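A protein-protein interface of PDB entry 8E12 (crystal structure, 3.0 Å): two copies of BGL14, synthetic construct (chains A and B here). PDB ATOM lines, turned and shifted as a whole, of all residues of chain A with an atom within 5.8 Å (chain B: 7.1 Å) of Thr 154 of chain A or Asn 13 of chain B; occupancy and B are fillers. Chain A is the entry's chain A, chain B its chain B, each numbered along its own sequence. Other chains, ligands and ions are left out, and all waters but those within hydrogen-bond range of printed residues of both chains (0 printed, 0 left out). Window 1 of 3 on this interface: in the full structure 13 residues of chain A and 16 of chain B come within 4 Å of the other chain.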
ATOM      1  N   ALA A 149     -17.793 -13.569  -9.513  1.00  0.00           N
ATOM      2  CA  ALA A 149     -18.460 -14.608  -8.740  1.00  0.00           C
ATOM      3  C   ALA A 149     -17.473 -15.668  -8.265  1.00  0.00           C
ATOM      4  O   ALA A 149     -17.518 -16.089  -7.103  1.00  0.00           O
ATOM      5  CB  ALA A 149     -19.572 -15.242  -9.574  1.00  0.00           C
ATOM      6  N   LEU A 150     -16.558 -16.095  -9.138  1.00  0.00           N
ATOM      7  CA  LEU A 150     -15.545 -17.057  -8.718  1.00  0.00           C
ATOM      8  C   LEU A 150     -14.588 -16.441  -7.709  1.00  0.00           C
ATOM      9  O   LEU A 150     -14.139 -17.118  -6.776  1.00  0.00           O
ATOM     10  CB  LEU A 150     -14.779 -17.589  -9.930  1.00  0.00           C
ATOM     11  CG  LEU A 150     -15.495 -18.583 -10.846  1.00  0.00           C
ATOM     12  CD1 LEU A 150     -14.492 -19.484 -11.545  1.00  0.00           C
ATOM     13  CD2 LEU A 150     -16.500 -19.416 -10.066  1.00  0.00           C
ATOM     14  N   ARG A 151     -14.260 -15.157  -7.878  1.00  0.00           N
ATOM     15  CA  ARG A 151     -13.477 -14.460  -6.865  1.00  0.00           C
ATOM     16  C   ARG A 151     -14.202 -14.449  -5.526  1.00  0.00           C
ATOM     17  O   ARG A 151     -13.594 -14.711  -4.481  1.00  0.00           O
ATOM     18  CB  ARG A 151     -13.169 -13.035  -7.324  1.00  0.00           C
ATOM     19  CG  ARG A 151     -11.842 -12.495  -6.818  1.00  0.00           C
ATOM     20  N   LEU A 152     -15.505 -14.158  -5.538  1.00  0.00           N
ATOM     21  CA  LEU A 152     -16.292 -14.236  -4.311  1.00  0.00           C
ATOM     22  C   LEU A 152     -16.386 -15.674  -3.818  1.00  0.00           C
ATOM     23  O   LEU A 152     -16.230 -15.943  -2.620  1.00  0.00           O
ATOM     24  CB  LEU A 152     -17.685 -13.649  -4.541  1.00  0.00           C
ATOM     25  CG  LEU A 152     -18.377 -13.049  -3.315  1.00  0.00           C
ATOM     26  N   HIS A 153     -16.674 -16.608  -4.731  1.00  0.00           N
ATOM     27  CA  HIS A 153     -16.790 -18.018  -4.370  1.00  0.00           C
ATOM     28  C   HIS A 153     -15.545 -18.504  -3.637  1.00  0.00           C
ATOM     29  O   HIS A 153     -15.641 -19.248  -2.653  1.00  0.00           O
ATOM     30  CB  HIS A 153     -17.053 -18.846  -5.633  1.00  0.00           C
ATOM     31  CG  HIS A 153     -17.182 -20.319  -5.395  1.00  0.00           C
ATOM     32  ND1 HIS A 153     -16.139 -21.100  -4.946  1.00  0.00           N
ATOM     33  CD2 HIS A 153     -18.235 -21.155  -5.557  1.00  0.00           C
ATOM     34  CE1 HIS A 153     -16.543 -22.352  -4.837  1.00  0.00           C
ATOM     35  NE2 HIS A 153     -17.811 -22.414  -5.202  1.00  0.00           N
ATOM     36  N   THR A 154     -14.363 -18.095  -4.108  1.00  0.00           N
ATOM     37  CA  THR A 154     -13.120 -18.465  -3.439  1.00  0.00           C
ATOM     38  C   THR A 154     -13.054 -17.892  -2.027  1.00  0.00           C
ATOM     39  O   THR A 154     -12.576 -18.556  -1.100  1.00  0.00           O
ATOM     40  CB  THR A 154     -11.925 -17.984  -4.261  1.00  0.00           C
ATOM     41  OG1 THR A 154     -12.010 -18.511  -5.590  1.00  0.00           O
ATOM     42  CG2 THR A 154     -10.631 -18.432  -3.618  1.00  0.00           C
ATOM     43  N   GLU A 155     -13.532 -16.659  -1.846  1.00  0.00           N
ATOM     44  CA  GLU A 155     -13.436 -16.008  -0.544  1.00  0.00           C
ATOM     45  C   GLU A 155     -14.322 -16.697   0.487  1.00  0.00           C
ATOM     46  O   GLU A 155     -13.977 -16.736   1.674  1.00  0.00           O
ATOM     47  CB  GLU A 155     -13.802 -14.530  -0.665  1.00  0.00           C
ATOM     48  CG  GLU A 155     -12.735 -13.592  -0.125  1.00  0.00           C
ATOM     49  CD  GLU A 155     -11.371 -13.849  -0.736  1.00  0.00           C
ATOM     50  N   ILE A 156     -15.465 -17.231   0.051  1.00  0.00           N
ATOM     51  CA  ILE A 156     -16.344 -17.990   0.938  1.00  0.00           C
ATOM     52  C   ILE A 156     -15.613 -19.196   1.515  1.00  0.00           C
ATOM     53  O   ILE A 156     -15.805 -19.558   2.682  1.00  0.00           O
ATOM     54  CB  ILE A 156     -17.613 -18.409   0.176  1.00  0.00           C
ATOM     55  CG1 ILE A 156     -18.311 -17.172  -0.393  1.00  0.00           C
ATOM     56  CG2 ILE A 156     -18.547 -19.200   1.081  1.00  0.00           C
ATOM     57  CD1 ILE A 156     -19.781 -17.356  -0.647  1.00  0.00           C
ATOM     58  N   MET A 157     -14.777 -19.846   0.702  1.00  0.00           N
ATOM     59  CA  MET A 157     -13.985 -20.973   1.187  1.00  0.00           C
ATOM     60  C   MET A 157     -13.104 -20.568   2.362  1.00  0.00           C
ATOM     61  O   MET A 157     -12.964 -21.326   3.330  1.00  0.00           O
ATOM     62  CB  MET A 157     -13.146 -21.542   0.046  1.00  0.00           C
ATOM     63  CG  MET A 157     -13.873 -22.605  -0.755  1.00  0.00           C
ATOM     64  SD  MET A 157     -12.853 -23.394  -2.008  1.00  0.00           S
ATOM     65  CE  MET A 157     -11.495 -22.243  -2.130  1.00  0.00           C
ATOM     66  N   ARG A 158     -12.492 -19.382   2.291  1.00  0.00           N
ATOM     67  CA  ARG A 158     -11.667 -18.904   3.396  1.00  0.00           C
ATOM     68  C   ARG A 158     -12.467 -18.824   4.692  1.00  0.00           C
ATOM     69  O   ARG A 158     -11.939 -19.106   5.774  1.00  0.00           O
ATOM     70  CB  ARG A 158     -11.060 -17.542   3.056  1.00  0.00           C
ATOM     71  CG  ARG A 158      -9.544 -17.489   3.175  1.00  0.00           C
ATOM     72  CD  ARG A 158      -9.064 -16.085   3.507  1.00  0.00           C
ATOM     73  N   LYS B   8     -15.987 -30.585  -0.395  1.00  0.00           N
ATOM     74  CA  LYS B   8     -16.730 -30.492  -1.648  1.00  0.00           C
ATOM     75  C   LYS B   8     -16.574 -29.111  -2.271  1.00  0.00           C
ATOM     76  O   LYS B   8     -16.371 -28.987  -3.484  1.00  0.00           O
ATOM     77  CB  LYS B   8     -18.205 -30.812  -1.411  1.00  0.00           C
ATOM     78  N   LEU B   9     -16.677 -28.063  -1.449  1.00  0.00           N
ATOM     79  CA  LEU B   9     -16.531 -26.698  -1.944  1.00  0.00           C
ATOM     80  C   LEU B   9     -15.125 -26.447  -2.474  1.00  0.00           C
ATOM     81  O   LEU B   9     -14.947 -25.722  -3.461  1.00  0.00           O
ATOM     82  CB  LEU B   9     -16.871 -25.702  -0.837  1.00  0.00           C
ATOM     83  CG  LEU B   9     -17.014 -24.252  -1.294  1.00  0.00           C
ATOM     84  CD1 LEU B   9     -18.036 -24.169  -2.415  1.00  0.00           C
ATOM     85  CD2 LEU B   9     -17.396 -23.344  -0.139  1.00  0.00           C
ATOM     86  N   LEU B  10     -14.112 -27.013  -1.814  1.00  0.00           N
ATOM     87  CA  LEU B  10     -12.740 -26.855  -2.286  1.00  0.00           C
ATOM     88  C   LEU B  10     -12.574 -27.434  -3.684  1.00  0.00           C
ATOM     89  O   LEU B  10     -12.018 -26.783  -4.576  1.00  0.00           O
ATOM     90  CB  LEU B  10     -11.767 -27.515  -1.309  1.00  0.00           C
ATOM     91  CG  LEU B  10     -10.298 -27.113  -1.446  1.00  0.00           C
ATOM     92  N   GLU B  11     -13.059 -28.661  -3.895  1.00  0.00           N
ATOM     93  CA  GLU B  11     -12.998 -29.268  -5.220  1.00  0.00           C
ATOM     94  C   GLU B  11     -13.888 -28.526  -6.210  1.00  0.00           C
ATOM     95  O   GLU B  11     -13.546 -28.406  -7.392  1.00  0.00           O
ATOM     96  CB  GLU B  11     -13.398 -30.741  -5.140  1.00  0.00           C
ATOM     97  N   GLU B  12     -15.041 -28.037  -5.748  1.00  0.00           N
ATOM     98  CA  GLU B  12     -15.941 -27.298  -6.627  1.00  0.00           C
ATOM     99  C   GLU B  12     -15.300 -26.010  -7.130  1.00  0.00           C
ATOM    100  O   GLU B  12     -15.498 -25.620  -8.286  1.00  0.00           O
ATOM    101  CB  GLU B  12     -17.249 -26.998  -5.896  1.00  0.00           C
ATOM    102  CG  GLU B  12     -18.365 -26.489  -6.792  1.00  0.00           C
ATOM    103  CD  GLU B  12     -19.673 -26.317  -6.046  1.00  0.00           C
ATOM    104  OE1 GLU B  12     -20.584 -25.652  -6.580  1.00  0.00           O
ATOM    105  OE2 GLU B  12     -19.788 -26.851  -4.922  1.00  0.00           O
ATOM    106  N   ASN B  13     -14.531 -25.331  -6.275  1.00  0.00           N
ATOM    107  CA  ASN B  13     -13.932 -24.059  -6.667  1.00  0.00           C
ATOM    108  C   ASN B  13     -12.867 -24.250  -7.741  1.00  0.00           C
ATOM    109  O   ASN B  13     -12.878 -23.557  -8.765  1.00  0.00           O
ATOM    110  CB  ASN B  13     -13.344 -23.362  -5.441  1.00  0.00           C
ATOM    111  CG  ASN B  13     -12.451 -22.190  -5.805  1.00  0.00           C
ATOM    112  OD1 ASN B  13     -11.244 -22.348  -5.987  1.00  0.00           O
ATOM    113  ND2 ASN B  13     -13.042 -21.005  -5.907  1.00  0.00           N
ATOM    114  N   ILE B  14     -11.939 -25.187  -7.529  1.00  0.00           N
ATOM    115  CA  ILE B  14     -10.865 -25.388  -8.497  1.00  0.00           C
ATOM    116  C   ILE B  14     -11.426 -25.902  -9.816  1.00  0.00           C
ATOM    117  O   ILE B  14     -10.936 -25.549 -10.895  1.00  0.00           O
ATOM    118  CB  ILE B  14      -9.788 -26.334  -7.934  1.00  0.00           C
ATOM    119  CG1 ILE B  14     -10.425 -27.485  -7.159  1.00  0.00           C
ATOM    120  CG2 ILE B  14      -8.832 -25.568  -7.034  1.00  0.00           C
ATOM    121  CD1 ILE B  14      -9.439 -28.557  -6.748  1.00  0.00           C
ATOM    122  N   LYS B  15     -12.454 -26.751  -9.751  1.00  0.00           N
ATOM    123  CA  LYS B  15     -13.068 -27.268 -10.970  1.00  0.00           C
ATOM    124  C   LYS B  15     -13.694 -26.141 -11.784  1.00  0.00           C
ATOM    125  O   LYS B  15     -13.509 -26.066 -13.004  1.00  0.00           O
ATOM    126  CB  LYS B  15     -14.113 -28.329 -10.622  1.00  0.00           C
ATOM    127  N   LEU B  16     -14.424 -25.242 -11.120  1.00  0.00           N
ATOM    128  CA  LEU B  16     -15.031 -24.122 -11.831  1.00  0.00           C
ATOM    129  C   LEU B  16     -13.964 -23.205 -12.415  1.00  0.00           C
ATOM    130  O   LEU B  16     -14.126 -22.676 -13.521  1.00  0.00           O
ATOM    131  CB  LEU B  16     -15.959 -23.348 -10.896  1.00  0.00           C
ATOM    132  CG  LEU B  16     -17.441 -23.717 -10.973  1.00  0.00           C
ATOM    133  N   ILE B  17     -12.865 -23.006 -11.684  1.00  0.00           N
ATOM    134  CA  ILE B  17     -11.778 -22.169 -12.182  1.00  0.00           C
ATOM    135  C   ILE B  17     -11.083 -22.847 -13.356  1.00  0.00           C
ATOM    136  O   ILE B  17     -10.801 -22.216 -14.382  1.00  0.00           O
ATOM    137  CB  ILE B  17     -10.788 -21.845 -11.048  1.00  0.00           C
ATOM    138  CG1 ILE B  17     -11.456 -20.959  -9.996  1.00  0.00           C
ATOM    139  CG2 ILE B  17      -9.547 -21.161 -11.603  1.00  0.00           C
ATOM    140  CD1 ILE B  17     -10.599 -20.711  -8.778  1.00  0.00           C
ATOM    141  N   GLU B  18     -10.784 -24.142 -13.217  1.00  0.00           N
ATOM    142  CA  GLU B  18     -10.084 -24.860 -14.278  1.00  0.00           C
ATOM    143  C   GLU B  18     -10.922 -24.922 -15.550  1.00  0.00           C
ATOM    144  O   GLU B  18     -10.393 -24.764 -16.657  1.00  0.00           O
ATOM    145  CB  GLU B  18      -9.715 -26.268 -13.808  1.00  0.00           C
ATOM    146  N   GLU B  19     -12.232 -25.154 -15.414  1.00  0.00           N
ATOM    147  CA  GLU B  19     -13.102 -25.145 -16.586  1.00  0.00           C
ATOM    148  C   GLU B  19     -13.146 -23.759 -17.217  1.00  0.00           C
ATOM    149  O   GLU B  19     -13.157 -23.628 -18.447  1.00  0.00           O
ATOM    150  CB  GLU B  19     -14.512 -25.616 -16.220  1.00  0.00           C
ATOM    151  CG  GLU B  19     -14.610 -27.090 -15.841  1.00  0.00           C
ATOM    152  CD  GLU B  19     -15.624 -27.349 -14.740  1.00  0.00           C
ATOM    153  OE1 GLU B  19     -16.821 -27.062 -14.955  1.00  0.00           O
ATOM    154  OE2 GLU B  19     -15.229 -27.847 -13.665  1.00  0.00           O
ATOM    155  N   VAL B  38      -7.632 -14.925 -10.021  1.00  0.00           N
ATOM    156  CA  VAL B  38      -8.450 -15.683  -9.081  1.00  0.00           C
ATOM    157  C   VAL B  38      -7.793 -17.019  -8.752  1.00  0.00           C
ATOM    158  O   VAL B  38      -7.881 -17.507  -7.618  1.00  0.00           O
ATOM    159  CB  VAL B  38      -9.870 -15.867  -9.650  1.00  0.00           C
ATOM    160  CG1 VAL B  38     -10.696 -16.796  -8.768  1.00  0.00           C
ATOM    161  CG2 VAL B  38     -10.557 -14.518  -9.811  1.00  0.00           C
ATOM    162  N   LEU B  39      -7.124 -17.630  -9.734  1.00  0.00           N
ATOM    163  CA  LEU B  39      -6.482 -18.922  -9.513  1.00  0.00           C
ATOM    164  C   LEU B  39      -5.412 -18.839  -8.428  1.00  0.00           C
ATOM    165  O   LEU B  39      -5.424 -19.621  -7.470  1.00  0.00           O
ATOM    166  CB  LEU B  39      -5.884 -19.438 -10.824  1.00  0.00           C
ATOM    167  CG  LEU B  39      -5.087 -20.743 -10.756  1.00  0.00           C
ATOM    168  CD1 LEU B  39      -5.864 -21.814  -9.999  1.00  0.00           C
ATOM    169  CD2 LEU B  39      -4.718 -21.228 -12.150  1.00  0.00           C
ATOM    170  N   ARG B  41      -5.114 -16.517  -6.241  1.00  0.00           N
ATOM    171  CA  ARG B  41      -5.818 -16.203  -5.003  1.00  0.00           C
ATOM    172  C   ARG B  41      -6.442 -17.458  -4.411  1.00  0.00           C
ATOM    173  O   ARG B  41      -6.439 -17.649  -3.189  1.00  0.00           O
ATOM    174  CB  ARG B  41      -6.885 -15.137  -5.258  1.00  0.00           C
ATOM    175  CG  ARG B  41      -6.974 -14.072  -4.173  1.00  0.00           C
ATOM    176  CD  ARG B  41      -7.524 -12.767  -4.725  1.00  0.00           C
ATOM    177  N   SER B  42      -6.984 -18.328  -5.268  1.00  0.00           N
ATOM    178  CA  SER B  42      -7.545 -19.587  -4.795  1.00  0.00           C
ATOM    179  C   SER B  42      -6.457 -20.534  -4.309  1.00  0.00           C
ATOM    180  O   SER B  42      -6.630 -21.209  -3.291  1.00  0.00           O
ATOM    181  CB  SER B  42      -8.373 -20.247  -5.896  1.00  0.00           C
ATOM    182  OG  SER B  42      -8.735 -21.568  -5.531  1.00  0.00           O
ATOM    183  N   VAL B  43      -5.326 -20.593  -5.019  1.00  0.00           N
ATOM    184  CA  VAL B  43      -4.274 -21.541  -4.660  1.00  0.00           C
ATOM    185  C   VAL B  43      -3.742 -21.265  -3.260  1.00  0.00           C
ATOM    186  O   VAL B  43      -3.387 -22.200  -2.530  1.00  0.00           O
ATOM    187  CB  VAL B  43      -3.148 -21.506  -5.717  1.00  0.00           C
ATOM    188  CG1 VAL B  43      -1.879 -22.173  -5.197  1.00  0.00           C
ATOM    189  CG2 VAL B  43      -3.605 -22.190  -6.997  1.00  0.00           C
ATOM    190  N   VAL B  45      -5.411 -20.314  -0.638  1.00  0.00           N
ATOM    191  CA  VAL B  45      -6.274 -20.912   0.373  1.00  0.00           C
ATOM    192  C   VAL B  45      -6.227 -22.436   0.306  1.00  0.00           C
ATOM    193  O   VAL B  45      -6.471 -23.105   1.315  1.00  0.00           O
ATOM    194  CB  VAL B  45      -7.713 -20.372   0.265  1.00  0.00           C
ATOM    195  CG1 VAL B  45      -7.701 -18.867   0.055  1.00  0.00           C
ATOM    196  CG2 VAL B  45      -8.478 -21.067  -0.834  1.00  0.00           C
ATOM    197  N   ILE B  46      -5.919 -23.019  -0.859  1.00  0.00           N
ATOM    198  CA  ILE B  46      -5.771 -24.472  -0.885  1.00  0.00           C
ATOM    199  C   ILE B  46      -4.490 -24.869  -0.166  1.00  0.00           C
ATOM    200  O   ILE B  46      -4.410 -25.953   0.427  1.00  0.00           O
ATOM    201  CB  ILE B  46      -5.800 -25.020  -2.326  1.00  0.00           C
ATOM    202  CG1 ILE B  46      -6.736 -24.206  -3.222  1.00  0.00           C
ATOM    203  CG2 ILE B  46      -6.218 -26.474  -2.337  1.00  0.00           C
ATOM    204  CD1 ILE B  46      -8.186 -24.218  -2.772  1.00  0.00           C
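OG1 of Thr 154 of chain A is in hydrogen-bond range of O of Leu 150 of chain A, at 2.8 Å.
The side-chain hydroxyl (OG) of Ser 42 of chain B is in hydrogen-bond range of the side-chain amide oxygen (OD1) of Asn 13 of chain B.
A ring nitrogen (ND1) of His 153 of chain A lies within hydrogen-bond range of the side-chain amide nitrogen (ND2) of Asn 13 of chain B, 3.2 Å away.
The side-chain hydroxyl of Thr 154 of chain A is in hydrogen-bond range of the side-chain amide nitrogen of Asn 13 of chain B, at 2.7 Å.
The side-chain sulfur of Met 157 of chain A lies close to the backbone carbonyl oxygen of Leu 9 of chain B (3.5 Å).
No position is printed for both chains.
Of the 15 pairs that touch across the chains among the printed residues, none has its exchanged pair printed and touching as well.
Printed residues of chain B that touch a printed residue of chain A: Leu 9, Leu 10, Asn 13, Leu 16, Ile 17, Val 38, Ser 42, Val 45 and Ile 46.
Hydrophobic or aromatic side chains of chain A that line the printed part of chain B: Leu 150, His 153 and Met 157.
Among the printed residues, no Asp or Glu carboxylate lies within 4 Å of a Lys or Arg side-chain nitrogen of the other chain.
Among the printed residues, pairs that only touch across the chains: Leu 150 of chain A with Leu 16 of chain B (3.8 Å), Leu 150 of chain A with Ile 17 of chain B (3.7 Å), Leu 150 of chain A with Val 38 of chain B (3.99 Å), Arg 151 of chain A with Val 38 of chain B (3.8 Å), His 153 of chain A with Leu 9 of chain B (3.3 Å), Thr 154 of chain A with Val 38 of chain B (3.8 Å), Thr 154 of chain A with Ser 42 of chain B (3.5 Å), Met 157 of chain A with Leu 10 of chain B (3.5 Å), Met 157 of chain A with Asn 13 of chain B (3.5 Å), Met 157 of chain A with Val 45 of chain B (3.5 Å), Met 157 of chain A with Ile 46 of chain B (3.9 Å) and Arg 158 of chain A with Val 45 of chain B (3.9 Å).
Asn 13 of chain B touches three residues of chain A.
Of the printed residues of chain B, Leu 150 of chain A touches Leu 16 (3.8 Å), Ile 17 (3.7 Å) and Val 38 (3.99 Å).
Of the printed residues of chain A, Ile 17 of chain B touches Leu 150 (3.7 Å).
Leu 39 of chain B touches none of the printed residues of chain A.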
